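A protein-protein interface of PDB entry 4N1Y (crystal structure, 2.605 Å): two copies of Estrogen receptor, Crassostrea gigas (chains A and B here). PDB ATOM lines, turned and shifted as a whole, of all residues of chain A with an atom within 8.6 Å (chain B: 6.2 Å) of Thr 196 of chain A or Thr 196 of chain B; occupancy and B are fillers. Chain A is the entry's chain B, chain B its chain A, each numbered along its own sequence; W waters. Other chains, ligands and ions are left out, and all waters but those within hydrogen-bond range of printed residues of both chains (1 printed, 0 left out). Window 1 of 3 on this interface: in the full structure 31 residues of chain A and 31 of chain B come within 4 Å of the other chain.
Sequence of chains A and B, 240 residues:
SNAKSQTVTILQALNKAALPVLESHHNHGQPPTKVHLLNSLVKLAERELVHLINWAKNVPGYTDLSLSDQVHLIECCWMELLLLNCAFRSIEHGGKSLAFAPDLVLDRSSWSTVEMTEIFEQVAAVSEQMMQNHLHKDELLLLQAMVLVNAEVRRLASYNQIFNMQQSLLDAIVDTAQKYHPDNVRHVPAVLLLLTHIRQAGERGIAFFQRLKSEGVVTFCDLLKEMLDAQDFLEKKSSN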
ATOM      1  N   GLU A  80     -21.421 -14.097   7.443  1.00  0.00           N
ATOM      2  CA  GLU A  80     -22.484 -14.734   8.221  1.00  0.00           C
ATOM      3  C   GLU A  80     -23.214 -13.680   9.047  1.00  0.00           C
ATOM      4  O   GLU A  80     -24.443 -13.650   9.098  1.00  0.00           O
ATOM      5  CB  GLU A  80     -21.933 -15.816   9.151  1.00  0.00           C
ATOM      6  CG  GLU A  80     -20.975 -16.793   8.509  1.00  0.00           C
ATOM      7  CD  GLU A  80     -20.334 -17.741   9.522  1.00  0.00           C
ATOM      8  OE1 GLU A  80     -21.064 -18.265  10.391  1.00  0.00           O
ATOM      9  OE2 GLU A  80     -19.091 -17.921   9.480  1.00  0.00           O
ATOM     10  N   LEU A  84     -27.021 -12.980   8.847  1.00  0.00           N
ATOM     11  CA  LEU A  84     -27.783 -13.230  10.060  1.00  0.00           C
ATOM     12  C   LEU A  84     -28.602 -12.001  10.417  1.00  0.00           C
ATOM     13  O   LEU A  84     -29.779 -12.111  10.755  1.00  0.00           O
ATOM     14  CB  LEU A  84     -26.871 -13.615  11.224  1.00  0.00           C
ATOM     15  CG  LEU A  84     -27.654 -13.806  12.518  1.00  0.00           C
ATOM     16  CD1 LEU A  84     -28.270 -15.177  12.504  1.00  0.00           C
ATOM     17  CD2 LEU A  84     -26.769 -13.647  13.739  1.00  0.00           C
ATOM     18  N   GLN A 122     -32.028 -19.261   1.055  1.00  0.00           N
ATOM     19  CA  GLN A 122     -31.656 -19.853   2.317  1.00  0.00           C
ATOM     20  C   GLN A 122     -31.826 -18.846   3.472  1.00  0.00           C
ATOM     21  O   GLN A 122     -32.369 -19.168   4.536  1.00  0.00           O
ATOM     22  CB  GLN A 122     -30.228 -20.376   2.227  1.00  0.00           C
ATOM     23  CG  GLN A 122     -29.828 -21.300   3.356  1.00  0.00           C
ATOM     24  CD  GLN A 122     -28.533 -22.016   3.067  1.00  0.00           C
ATOM     25  OE1 GLN A 122     -27.678 -21.509   2.337  1.00  0.00           O
ATOM     26  NE2 GLN A 122     -28.392 -23.221   3.604  1.00  0.00           N
ATOM     27  N   VAL A 126     -34.437 -18.862   6.622  1.00  0.00           N
ATOM     28  CA  VAL A 126     -33.963 -18.703   7.979  1.00  0.00           C
ATOM     29  C   VAL A 126     -34.778 -17.605   8.648  1.00  0.00           C
ATOM     30  O   VAL A 126     -35.207 -17.765   9.796  1.00  0.00           O
ATOM     31  CB  VAL A 126     -32.452 -18.365   8.031  1.00  0.00           C
ATOM     32  CG1 VAL A 126     -32.097 -17.732   9.357  1.00  0.00           C
ATOM     33  CG2 VAL A 126     -31.593 -19.612   7.764  1.00  0.00           C
ATOM     34  N   MET A 146     -22.396 -15.068  19.333  1.00  0.00           N
ATOM     35  CA  MET A 146     -22.082 -16.473  19.184  1.00  0.00           C
ATOM     36  C   MET A 146     -21.485 -16.784  17.806  1.00  0.00           C
ATOM     37  O   MET A 146     -20.479 -17.488  17.702  1.00  0.00           O
ATOM     38  CB  MET A 146     -23.343 -17.301  19.408  1.00  0.00           C
ATOM     39  CG  MET A 146     -23.065 -18.757  19.477  1.00  0.00           C
ATOM     40  SD  MET A 146     -21.724 -19.059  20.628  1.00  0.00           S
ATOM     41  CE  MET A 146     -22.664 -19.215  22.127  1.00  0.00           C
ATOM     42  N   VAL A 147     -22.071 -16.212  16.757  1.00  0.00           N
ATOM     43  CA  VAL A 147     -21.585 -16.430  15.393  1.00  0.00           C
ATOM     44  C   VAL A 147     -20.124 -16.006  15.309  1.00  0.00           C
ATOM     45  O   VAL A 147     -19.300 -16.681  14.701  1.00  0.00           O
ATOM     46  CB  VAL A 147     -22.415 -15.655  14.350  1.00  0.00           C
ATOM     47  CG1 VAL A 147     -21.734 -15.720  12.965  1.00  0.00           C
ATOM     48  CG2 VAL A 147     -23.806 -16.235  14.259  1.00  0.00           C
ATOM     49  N   ASN A 150     -17.839 -18.359  17.482  1.00  0.00           N
ATOM     50  CA  ASN A 150     -17.867 -19.709  16.921  1.00  0.00           C
ATOM     51  C   ASN A 150     -17.287 -19.709  15.507  1.00  0.00           C
ATOM     52  O   ASN A 150     -17.354 -20.718  14.796  1.00  0.00           O
ATOM     53  CB  ASN A 150     -19.293 -20.247  16.872  1.00  0.00           C
ATOM     54  CG  ASN A 150     -19.349 -21.757  16.679  1.00  0.00           C
ATOM     55  OD1 ASN A 150     -18.642 -22.502  17.365  1.00  0.00           O
ATOM     56  ND2 ASN A 150     -20.162 -22.217  15.716  1.00  0.00           N
ATOM     57  N   ALA A 151     -16.717 -18.574  15.101  1.00  0.00           N
ATOM     58  CA  ALA A 151     -16.232 -18.425  13.730  1.00  0.00           C
ATOM     59  C   ALA A 151     -15.185 -19.472  13.369  1.00  0.00           C
ATOM     60  O   ALA A 151     -15.279 -20.120  12.335  1.00  0.00           O
ATOM     61  CB  ALA A 151     -15.665 -17.030  13.513  1.00  0.00           C
ATOM     62  N   GLU A 152     -14.213 -19.675  14.248  1.00  0.00           N
ATOM     63  CA  GLU A 152     -13.109 -20.566  13.921  1.00  0.00           C
ATOM     64  C   GLU A 152     -13.157 -21.706  14.898  1.00  0.00           C
ATOM     65  O   GLU A 152     -13.322 -21.483  16.093  1.00  0.00           O
ATOM     66  CB  GLU A 152     -11.766 -19.832  13.994  1.00  0.00           C
ATOM     67  CG  GLU A 152     -10.562 -20.722  13.820  1.00  0.00           C
ATOM     68  CD  GLU A 152     -10.433 -21.302  12.417  1.00  0.00           C
ATOM     69  OE1 GLU A 152     -10.777 -22.488  12.219  1.00  0.00           O
ATOM     70  OE2 GLU A 152      -9.969 -20.575  11.513  1.00  0.00           O
ATOM     71  N   VAL A 153     -13.070 -22.929  14.392  1.00  0.00           N
ATOM     72  CA  VAL A 153     -13.130 -24.096  15.264  1.00  0.00           C
ATOM     73  C   VAL A 153     -11.738 -24.655  15.537  1.00  0.00           C
ATOM     74  O   VAL A 153     -11.530 -25.385  16.506  1.00  0.00           O
ATOM     75  CB  VAL A 153     -14.025 -25.203  14.670  1.00  0.00           C
ATOM     76  CG1 VAL A 153     -13.390 -25.839  13.414  1.00  0.00           C
ATOM     77  CG2 VAL A 153     -14.361 -26.247  15.737  1.00  0.00           C
ATOM     78  N   PRO A 189     -32.097 -25.378  21.013  1.00  0.00           N
ATOM     79  CA  PRO A 189     -31.545 -26.230  19.954  1.00  0.00           C
ATOM     80  C   PRO A 189     -32.080 -25.875  18.560  1.00  0.00           C
ATOM     81  O   PRO A 189     -31.268 -25.787  17.635  1.00  0.00           O
ATOM     82  CB  PRO A 189     -31.972 -27.633  20.377  1.00  0.00           C
ATOM     83  CG  PRO A 189     -32.121 -27.530  21.869  1.00  0.00           C
ATOM     84  CD  PRO A 189     -32.672 -26.177  22.112  1.00  0.00           C
ATOM     85  N   ALA A 190     -33.387 -25.675  18.397  1.00  0.00           N
ATOM     86  CA  ALA A 190     -33.911 -25.368  17.068  1.00  0.00           C
ATOM     87  C   ALA A 190     -33.228 -24.132  16.511  1.00  0.00           C
ATOM     88  O   ALA A 190     -32.807 -24.117  15.350  1.00  0.00           O
ATOM     89  CB  ALA A 190     -35.403 -25.153  17.106  1.00  0.00           C
ATOM     90  N   VAL A 191     -33.100 -23.103  17.345  1.00  0.00           N
ATOM     91  CA  VAL A 191     -32.560 -21.826  16.882  1.00  0.00           C
ATOM     92  C   VAL A 191     -31.092 -21.956  16.528  1.00  0.00           C
ATOM     93  O   VAL A 191     -30.647 -21.479  15.484  1.00  0.00           O
ATOM     94  CB  VAL A 191     -32.746 -20.722  17.920  1.00  0.00           C
ATOM     95  CG1 VAL A 191     -31.972 -19.494  17.506  1.00  0.00           C
ATOM     96  CG2 VAL A 191     -34.220 -20.387  18.058  1.00  0.00           C
ATOM     97  N   LEU A 192     -30.339 -22.645  17.368  1.00  0.00           N
ATOM     98  CA  LEU A 192     -28.949 -22.904  17.038  1.00  0.00           C
ATOM     99  C   LEU A 192     -28.826 -23.634  15.695  1.00  0.00           C
ATOM    100  O   LEU A 192     -27.922 -23.354  14.916  1.00  0.00           O
ATOM    101  CB  LEU A 192     -28.309 -23.716  18.157  1.00  0.00           C
ATOM    102  CG  LEU A 192     -28.172 -22.826  19.393  1.00  0.00           C
ATOM    103  CD1 LEU A 192     -27.403 -23.513  20.461  1.00  0.00           C
ATOM    104  CD2 LEU A 192     -27.517 -21.492  19.007  1.00  0.00           C
ATOM    105  N   LEU A 193     -29.780 -24.509  15.387  1.00  0.00           N
ATOM    106  CA  LEU A 193     -29.743 -25.236  14.123  1.00  0.00           C
ATOM    107  C   LEU A 193     -29.833 -24.289  12.932  1.00  0.00           C
ATOM    108  O   LEU A 193     -29.339 -24.605  11.858  1.00  0.00           O
ATOM    109  CB  LEU A 193     -30.884 -26.247  14.034  1.00  0.00           C
ATOM    110  CG  LEU A 193     -30.825 -27.527  14.863  1.00  0.00           C
ATOM    111  CD1 LEU A 193     -32.061 -28.373  14.590  1.00  0.00           C
ATOM    112  CD2 LEU A 193     -29.559 -28.308  14.584  1.00  0.00           C
ATOM    113  N   LEU A 194     -30.434 -23.120  13.133  1.00  0.00           N
ATOM    114  CA  LEU A 194     -30.474 -22.135  12.069  1.00  0.00           C
ATOM    115  C   LEU A 194     -29.084 -21.688  11.681  1.00  0.00           C
ATOM    116  O   LEU A 194     -28.815 -21.411  10.504  1.00  0.00           O
ATOM    117  CB  LEU A 194     -31.280 -20.913  12.474  1.00  0.00           C
ATOM    118  CG  LEU A 194     -32.749 -21.202  12.706  1.00  0.00           C
ATOM    119  CD1 LEU A 194     -33.468 -19.918  13.101  1.00  0.00           C
ATOM    120  CD2 LEU A 194     -33.357 -21.841  11.480  1.00  0.00           C
ATOM    121  N   LEU A 195     -28.189 -21.659  12.663  1.00  0.00           N
ATOM    122  CA  LEU A 195     -26.841 -21.178  12.404  1.00  0.00           C
ATOM    123  C   LEU A 195     -26.117 -21.993  11.362  1.00  0.00           C
ATOM    124  O   LEU A 195     -25.315 -21.443  10.613  1.00  0.00           O
ATOM    125  CB  LEU A 195     -26.008 -21.144  13.679  1.00  0.00           C
ATOM    126  CG  LEU A 195     -26.364 -20.078  14.711  1.00  0.00           C
ATOM    127  CD1 LEU A 195     -25.365 -20.158  15.874  1.00  0.00           C
ATOM    128  CD2 LEU A 195     -26.377 -18.688  14.104  1.00  0.00           C
ATOM    129  N   THR A 196     -26.405 -23.288  11.287  1.00  0.00           N
ATOM    130  CA  THR A 196     -25.790 -24.102  10.252  1.00  0.00           C
ATOM    131  C   THR A 196     -26.167 -23.572   8.850  1.00  0.00           C
ATOM    132  O   THR A 196     -25.354 -23.630   7.927  1.00  0.00           O
ATOM    133  CB  THR A 196     -26.187 -25.560  10.357  1.00  0.00           C
ATOM    134  OG1 THR A 196     -27.558 -25.691   9.975  1.00  0.00           O
ATOM    135  CG2 THR A 196     -25.996 -26.076  11.787  1.00  0.00           C
ATOM    136  N   HIS A 197     -27.391 -23.073   8.679  1.00  0.00           N
ATOM    137  CA  HIS A 197     -27.790 -22.567   7.361  1.00  0.00           C
ATOM    138  C   HIS A 197     -27.153 -21.222   7.063  1.00  0.00           C
ATOM    139  O   HIS A 197     -26.760 -20.945   5.923  1.00  0.00           O
ATOM    140  CB  HIS A 197     -29.313 -22.503   7.255  1.00  0.00           C
ATOM    141  CG  HIS A 197     -29.946 -23.847   7.394  1.00  0.00           C
ATOM    142  ND1 HIS A 197     -29.773 -24.839   6.455  1.00  0.00           N
ATOM    143  CD2 HIS A 197     -30.649 -24.406   8.411  1.00  0.00           C
ATOM    144  CE1 HIS A 197     -30.383 -25.940   6.865  1.00  0.00           C
ATOM    145  NE2 HIS A 197     -30.911 -25.709   8.053  1.00  0.00           N
ATOM    146  N   ILE A 198     -27.057 -20.386   8.086  1.00  0.00           N
ATOM    147  CA  ILE A 198     -26.388 -19.102   7.970  1.00  0.00           C
ATOM    148  C   ILE A 198     -24.922 -19.284   7.566  1.00  0.00           C
ATOM    149  O   ILE A 198     -24.389 -18.529   6.755  1.00  0.00           O
ATOM    150  CB  ILE A 198     -26.487 -18.335   9.275  1.00  0.00           C
ATOM    151  CG1 ILE A 198     -27.888 -17.722   9.414  1.00  0.00           C
ATOM    152  CG2 ILE A 198     -25.452 -17.235   9.327  1.00  0.00           C
ATOM    153  CD1 ILE A 198     -28.166 -16.595   8.412  1.00  0.00           C
ATOM    154  N   ARG A 199     -24.280 -20.292   8.145  1.00  0.00           N
ATOM    155  CA  ARG A 199     -22.906 -20.638   7.810  1.00  0.00           C
ATOM    156  C   ARG A 199     -22.784 -21.052   6.337  1.00  0.00           C
ATOM    157  O   ARG A 199     -21.886 -20.607   5.620  1.00  0.00           O
ATOM    158  CB  ARG A 199     -22.420 -21.763   8.723  1.00  0.00           C
ATOM    159  CG  ARG A 199     -21.056 -22.332   8.375  1.00  0.00           C
ATOM    160  CD  ARG A 199     -19.941 -21.347   8.708  1.00  0.00           C
ATOM    161  NE  ARG A 199     -19.873 -20.985  10.129  1.00  0.00           N
ATOM    162  CZ  ARG A 199     -19.087 -21.576  11.033  1.00  0.00           C
ATOM    163  NH1 ARG A 199     -18.316 -22.603  10.684  1.00  0.00           N
ATOM    164  NH2 ARG A 199     -19.089 -21.160  12.298  1.00  0.00           N
ATOM    165  N   GLN A 200     -23.700 -21.900   5.887  1.00  0.00           N
ATOM    166  CA  GLN A 200     -23.720 -22.333   4.500  1.00  0.00           C
ATOM    167  C   GLN A 200     -23.973 -21.126   3.584  1.00  0.00           C
ATOM    168  O   GLN A 200     -23.299 -20.940   2.565  1.00  0.00           O
ATOM    169  CB  GLN A 200     -24.768 -23.422   4.298  1.00  0.00           C
ATOM    170  CG  GLN A 200     -24.769 -24.001   2.907  1.00  0.00           C
ATOM    171  CD  GLN A 200     -25.637 -25.230   2.797  1.00  0.00           C
ATOM    172  OE1 GLN A 200     -26.594 -25.402   3.549  1.00  0.00           O
ATOM    173  NE2 GLN A 200     -25.300 -26.103   1.861  1.00  0.00           N
ATOM    174  N   ALA A 201     -24.934 -20.294   3.961  1.00  0.00           N
ATOM    175  CA  ALA A 201     -25.207 -19.098   3.182  1.00  0.00           C
ATOM    176  C   ALA A 201     -23.994 -18.163   3.146  1.00  0.00           C
ATOM    177  O   ALA A 201     -23.699 -17.555   2.116  1.00  0.00           O
ATOM    178  CB  ALA A 201     -26.419 -18.367   3.739  1.00  0.00           C
ATOM    179  N   GLY A 202     -23.286 -18.058   4.262  1.00  0.00           N
ATOM    180  CA  GLY A 202     -22.138 -17.172   4.350  1.00  0.00           C
ATOM    181  C   GLY A 202     -21.060 -17.575   3.375  1.00  0.00           C
ATOM    182  O   GLY A 202     -20.507 -16.744   2.643  1.00  0.00           O
ATOM    183  N   GLU A 203     -20.781 -18.871   3.357  1.00  0.00           N
ATOM    184  CA  GLU A 203     -19.735 -19.442   2.519  1.00  0.00           C
ATOM    185  C   GLU A 203     -20.005 -19.161   1.053  1.00  0.00           C
ATOM    186  O   GLU A 203     -19.114 -18.738   0.292  1.00  0.00           O
ATOM    187  CB  GLU A 203     -19.650 -20.941   2.775  1.00  0.00           C
ATOM    188  CG  GLU A 203     -18.599 -21.705   2.010  1.00  0.00           C
ATOM    189  CD  GLU A 203     -17.247 -21.624   2.677  1.00  0.00           C
ATOM    190  OE1 GLU A 203     -17.138 -20.966   3.731  1.00  0.00           O
ATOM    191  OE2 GLU A 203     -16.300 -22.252   2.167  1.00  0.00           O
ATOM    192  N   GLN B 122     -10.674 -28.922   9.715  1.00  0.00           N
ATOM    193  CA  GLN B 122     -11.970 -28.565  10.295  1.00  0.00           C
ATOM    194  C   GLN B 122     -12.642 -29.807  10.903  1.00  0.00           C
ATOM    195  O   GLN B 122     -13.132 -29.776  12.037  1.00  0.00           O
ATOM    196  CB  GLN B 122     -12.851 -27.916   9.237  1.00  0.00           C
ATOM    197  CG  GLN B 122     -14.059 -27.187   9.768  1.00  0.00           C
ATOM    198  CD  GLN B 122     -14.752 -26.372   8.683  1.00  0.00           C
ATOM    199  OE1 GLN B 122     -14.670 -26.705   7.500  1.00  0.00           O
ATOM    200  NE2 GLN B 122     -15.446 -25.311   9.082  1.00  0.00           N
ATOM    201  N   ASN B 150     -32.072 -31.749   9.097  1.00  0.00           N
ATOM    202  CA  ASN B 150     -31.758 -30.319   9.028  1.00  0.00           C
ATOM    203  C   ASN B 150     -31.064 -29.929   7.736  1.00  0.00           C
ATOM    204  O   ASN B 150     -30.667 -28.780   7.558  1.00  0.00           O
ATOM    205  CB  ASN B 150     -30.893 -29.924  10.220  1.00  0.00           C
ATOM    206  CG  ASN B 150     -30.763 -28.430  10.385  1.00  0.00           C
ATOM    207  OD1 ASN B 150     -31.734 -27.696  10.241  1.00  0.00           O
ATOM    208  ND2 ASN B 150     -29.557 -27.970  10.738  1.00  0.00           N
ATOM    209  N   LEU B 192     -24.392 -28.811  19.386  1.00  0.00           N
ATOM    210  CA  LEU B 192     -25.076 -28.440  18.161  1.00  0.00           C
ATOM    211  C   LEU B 192     -24.263 -27.446  17.348  1.00  0.00           C
ATOM    212  O   LEU B 192     -24.314 -27.490  16.128  1.00  0.00           O
ATOM    213  CB  LEU B 192     -26.458 -27.881  18.466  1.00  0.00           C
ATOM    214  CG  LEU B 192     -27.361 -29.004  18.958  1.00  0.00           C
ATOM    215  CD1 LEU B 192     -28.773 -28.529  19.079  1.00  0.00           C
ATOM    216  CD2 LEU B 192     -27.263 -30.207  18.036  1.00  0.00           C
ATOM    217  N   LEU B 193     -23.505 -26.570  18.013  1.00  0.00           N
ATOM    218  CA  LEU B 193     -22.665 -25.594  17.307  1.00  0.00           C
ATOM    219  C   LEU B 193     -21.574 -26.237  16.465  1.00  0.00           C
ATOM    220  O   LEU B 193     -21.066 -25.627  15.521  1.00  0.00           O
ATOM    221  CB  LEU B 193     -22.007 -24.622  18.271  1.00  0.00           C
ATOM    222  CG  LEU B 193     -22.942 -23.578  18.851  1.00  0.00           C
ATOM    223  CD1 LEU B 193     -22.138 -22.662  19.737  1.00  0.00           C
ATOM    224  CD2 LEU B 193     -23.675 -22.829  17.747  1.00  0.00           C
ATOM    225  N   LEU B 194     -21.198 -27.457  16.818  1.00  0.00           N
ATOM    226  CA  LEU B 194     -20.262 -28.202  16.001  1.00  0.00           C
ATOM    227  C   LEU B 194     -20.837 -28.439  14.605  1.00  0.00           C
ATOM    228  O   LEU B 194     -20.086 -28.508  13.623  1.00  0.00           O
ATOM    229  CB  LEU B 194     -19.917 -29.527  16.660  1.00  0.00           C
ATOM    230  CG  LEU B 194     -19.121 -29.380  17.950  1.00  0.00           C
ATOM    231  CD1 LEU B 194     -18.880 -30.743  18.543  1.00  0.00           C
ATOM    232  CD2 LEU B 194     -17.799 -28.682  17.633  1.00  0.00           C
ATOM    233  N   LEU B 195     -22.164 -28.543  14.514  1.00  0.00           N
ATOM    234  CA  LEU B 195     -22.818 -28.812  13.235  1.00  0.00           C
ATOM    235  C   LEU B 195     -22.550 -27.744  12.188  1.00  0.00           C
ATOM    236  O   LEU B 195     -22.469 -28.059  11.006  1.00  0.00           O
ATOM    237  CB  LEU B 195     -24.314 -28.961  13.441  1.00  0.00           C
ATOM    238  CG  LEU B 195     -24.530 -30.254  14.210  1.00  0.00           C
ATOM    239  CD1 LEU B 195     -25.993 -30.454  14.560  1.00  0.00           C
ATOM    240  CD2 LEU B 195     -24.057 -31.377  13.330  1.00  0.00           C
ATOM    241  N   THR B 196     -22.384 -26.495  12.604  1.00  0.00           N
ATOM    242  CA  THR B 196     -22.039 -25.453  11.644  1.00  0.00           C
ATOM    243  C   THR B 196     -20.688 -25.723  10.963  1.00  0.00           C
ATOM    244  O   THR B 196     -20.540 -25.474   9.771  1.00  0.00           O
ATOM    245  CB  THR B 196     -21.970 -24.090  12.297  1.00  0.00           C
ATOM    246  OG1 THR B 196     -20.784 -24.013  13.092  1.00  0.00           O
ATOM    247  CG2 THR B 196     -23.210 -23.864  13.163  1.00  0.00           C
ATOM    248  N   HIS B 197     -19.712 -26.238  11.710  1.00  0.00           N
ATOM    249  CA  HIS B 197     -18.375 -26.496  11.146  1.00  0.00           C
ATOM    250  C   HIS B 197     -18.402 -27.699  10.237  1.00  0.00           C
ATOM    251  O   HIS B 197     -17.728 -27.729   9.208  1.00  0.00           O
ATOM    252  CB  HIS B 197     -17.318 -26.688  12.244  1.00  0.00           C
ATOM    253  CG  HIS B 197     -17.160 -25.486  13.124  1.00  0.00           C
ATOM    254  ND1 HIS B 197     -16.688 -24.279  12.651  1.00  0.00           N
ATOM    255  CD2 HIS B 197     -17.434 -25.293  14.436  1.00  0.00           C
ATOM    256  CE1 HIS B 197     -16.688 -23.391  13.629  1.00  0.00           C
ATOM    257  NE2 HIS B 197     -17.135 -23.981  14.721  1.00  0.00           N
ATOM    258  N   ILE B 198     -19.164 -28.706  10.634  1.00  0.00           N
ATOM    259  CA  ILE B 198     -19.366 -29.864   9.784  1.00  0.00           C
ATOM    260  C   ILE B 198     -20.009 -29.438   8.465  1.00  0.00           C
ATOM    261  O   ILE B 198     -19.652 -29.938   7.401  1.00  0.00           O
ATOM    262  CB  ILE B 198     -20.219 -30.908  10.489  1.00  0.00           C
ATOM    263  CG1 ILE B 198     -19.351 -31.651  11.504  1.00  0.00           C
ATOM    264  CG2 ILE B 198     -20.774 -31.886   9.508  1.00  0.00           C
ATOM    265  CD1 ILE B 198     -18.283 -32.520  10.853  1.00  0.00           C
ATOM    266  N   ARG B 199     -20.957 -28.511   8.531  1.00  0.00           N
ATOM    267  CA  ARG B 199     -21.603 -28.026   7.320  1.00  0.00           C
ATOM    268  C   ARG B 199     -20.583 -27.333   6.401  1.00  0.00           C
ATOM    269  O   ARG B 199     -20.522 -27.597   5.204  1.00  0.00           O
ATOM    270  CB  ARG B 199     -22.750 -27.075   7.675  1.00  0.00           C
ATOM    271  CG  ARG B 199     -23.448 -26.394   6.498  1.00  0.00           C
ATOM    272  CD  ARG B 199     -24.346 -27.377   5.762  1.00  0.00           C
ATOM    273  NE  ARG B 199     -25.413 -27.893   6.622  1.00  0.00           N
ATOM    274  CZ  ARG B 199     -26.646 -27.391   6.682  1.00  0.00           C
ATOM    275  NH1 ARG B 199     -26.980 -26.342   5.937  1.00  0.00           N
ATOM    276  NH2 ARG B 199     -27.544 -27.930   7.502  1.00  0.00           N
ATOM    277  N   GLN B 200     -19.753 -26.475   6.969  1.00  0.00           N
ATOM    278  CA  GLN B 200     -18.778 -25.779   6.162  1.00  0.00           C
ATOM    279  C   GLN B 200     -17.822 -26.775   5.511  1.00  0.00           C
ATOM    280  O   GLN B 200     -17.500 -26.656   4.332  1.00  0.00           O
ATOM    281  CB  GLN B 200     -18.023 -24.759   6.994  1.00  0.00           C
ATOM    282  CG  GLN B 200     -17.084 -23.907   6.180  1.00  0.00           C
ATOM    283  CD  GLN B 200     -16.531 -22.763   7.001  1.00  0.00           C
ATOM    284  OE1 GLN B 200     -16.436 -22.857   8.218  1.00  0.00           O
ATOM    285  NE2 GLN B 200     -16.168 -21.676   6.341  1.00  0.00           N
ATOM    286  N   ALA B 201     -17.358 -27.749   6.280  1.00  0.00           N
ATOM    287  CA  ALA B 201     -16.473 -28.770   5.728  1.00  0.00           C
ATOM    288  C   ALA B 201     -17.159 -29.629   4.662  1.00  0.00           C
ATOM    289  O   ALA B 201     -16.532 -30.033   3.673  1.00  0.00           O
ATOM    290  CB  ALA B 201     -15.933 -29.644   6.829  1.00  0.00           C
HETATM  291  O   HOH W   1     -17.850 -24.731  17.949  1.00  0.00           O
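The side-chain amide oxygen (OE1) of Gln 122 of chain B lies within hydrogen-bond range of the backbone NH (N) of Ala 201 of chain B.
The backbone carbonyl oxygen (O) of Leu 193 of chain B sits at hydrogen-bond distance from the side-chain hydroxyl (OG1) of Thr 196 of chain B (2.9 Å).
NE2 of Gln 122 of chain B lies close to O of His 197 of chain B (3.3 Å).
Water W1 bridges the side-chain amide oxygen of Asn 150 of chain A (2.4 Å) and a ring nitrogen (NE2) of His 197 of chain B (3.4 Å).
Glu 80 of chain A touches none of the printed residues of chain B.
Printed residues of chain B within 4 Å of Asn 150 of chain A: Leu 193, Thr 196 and His 197.
Of chain B, only Asn 150, Leu 195, Thr 196 and Arg 199 come within 4 Å of Thr 196 of chain A.
Printed residues of chain B within 4 Å of Gln 200 of chain A: Arg 199 (2.6 Å).
Of the printed residues of chain A, Gln 122 of chain B touches Val 153.
Thr 196 of chain B touches just these residues of chain A: Asn 150 (3.2 Å), Leu 195 (3.9 Å), Thr 196 (3.7 Å) and Arg 199 (3.4 Å).
His 197 of chain B touches just these residues of chain A: Asn 150, Ala 151, Val 153 and Arg 199.
The nearest residue of chain B that does not touch Thr 196 of chain A is Leu 192 of chain B (4.9 Å).
The nearest residue of chain A that does not touch Thr 196 of chain B is Leu 192 of chain A (5.1 Å).
The nearest printed residue of chain B that does not touch Pro 189 of chain A is Asn 150 of chain B (7.4 Å).
Leu 195 of chain A touches Leu 193 of chain B, but with the chains exchanged Leu 193 of chain A does not touch Leu 195 of chain B (4.2 Å).
Thr 196 of chain B touches its own counterpart, Thr 196 of chain A.
Thr 196 of chain A touches Arg 199 of chain B, and with the chains exchanged Arg 199 of chain A touches Thr 196 of chain B.
Positions printed for both chains: 122, 150, 192, 193, 194, 195, 196, 197, 198, 199, 200 and 201.
SD of Met 146 of chain A touches CD1 of Leu 193 of chain B (3.7 Å).
Ala 151 of chain A touches His 197 of chain B.
Gln 122 of chain B touches Val 153 of chain A (CG to CG1, 3.9 Å).
Val 153 of chain A touches His 197 of chain B.
Leu 193 of chain B touches Leu 195 of chain A (CD2 to CD1, 3.7 Å).
CG2 of Thr 196 of chain B touches C of Leu 195 of chain A, 3.9 Å away.
Thr 196 of chain A touches Leu 195 of chain B (CG2 to CB, 3.7 Å).
NE2 of His 197 of chain B sits close to O of Asn 150 of chain A (3.3 Å).
NH2 of Arg 199 of chain A sits at hydrogen-bond distance from OG1 of Thr 196 of chain B (3.4 Å).
OE1 of Gln 200 of chain B lies within hydrogen-bond range of NH1 of Arg 199 of chain A.
The side-chain hydroxyl of Thr 196 of chain B lies within hydrogen-bond range of the side-chain amide nitrogen of Asn 150 of chain A (3.2 Å).
The guanidinium group (NH1) of Arg 199 of chain B lies within hydrogen-bond range of the side-chain amide oxygen (OE1) of Gln 200 of chain A.
OG1 of Thr 196 of chain A sits at hydrogen-bond distance from ND2 of Asn 150 of chain B, 3.1 Å away.
NE2 of Gln 200 of chain B sits at hydrogen-bond distance from OE1 of Glu 203 of chain A (2.9 Å).
NH1 of Arg 199 of chain B is in hydrogen-bond range of ND1 of His 197 of chain A, at 3.2 Å.
NE2 of His 197 of chain A lies within hydrogen-bond range of OD1 of Asn 150 of chain B (3.1 Å).
The guanidinium group (NH2) of Arg 199 of chain B sits at hydrogen-bond distance from the side-chain hydroxyl (OG1) of Thr 196 of chain A (3.3 Å).
A ring nitrogen (ND1) of His 197 of chain B lies within hydrogen-bond range of the guanidinium group (NH1) of Arg 199 of chain A (3.1 Å).
Of the 12 printed residues of chain B, 9 touch a printed residue of chain A.
Hydrophobic or aromatic side chains of chain B within 4 Å of the printed part of chain A: Leu 192, Leu 193, Leu 195 and His 197.
Hydrophobic or aromatic side chains of chain A that line the printed part of chain B: Met 146, Val 153, Pro 189, Leu 193, Leu 195 and His 197.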
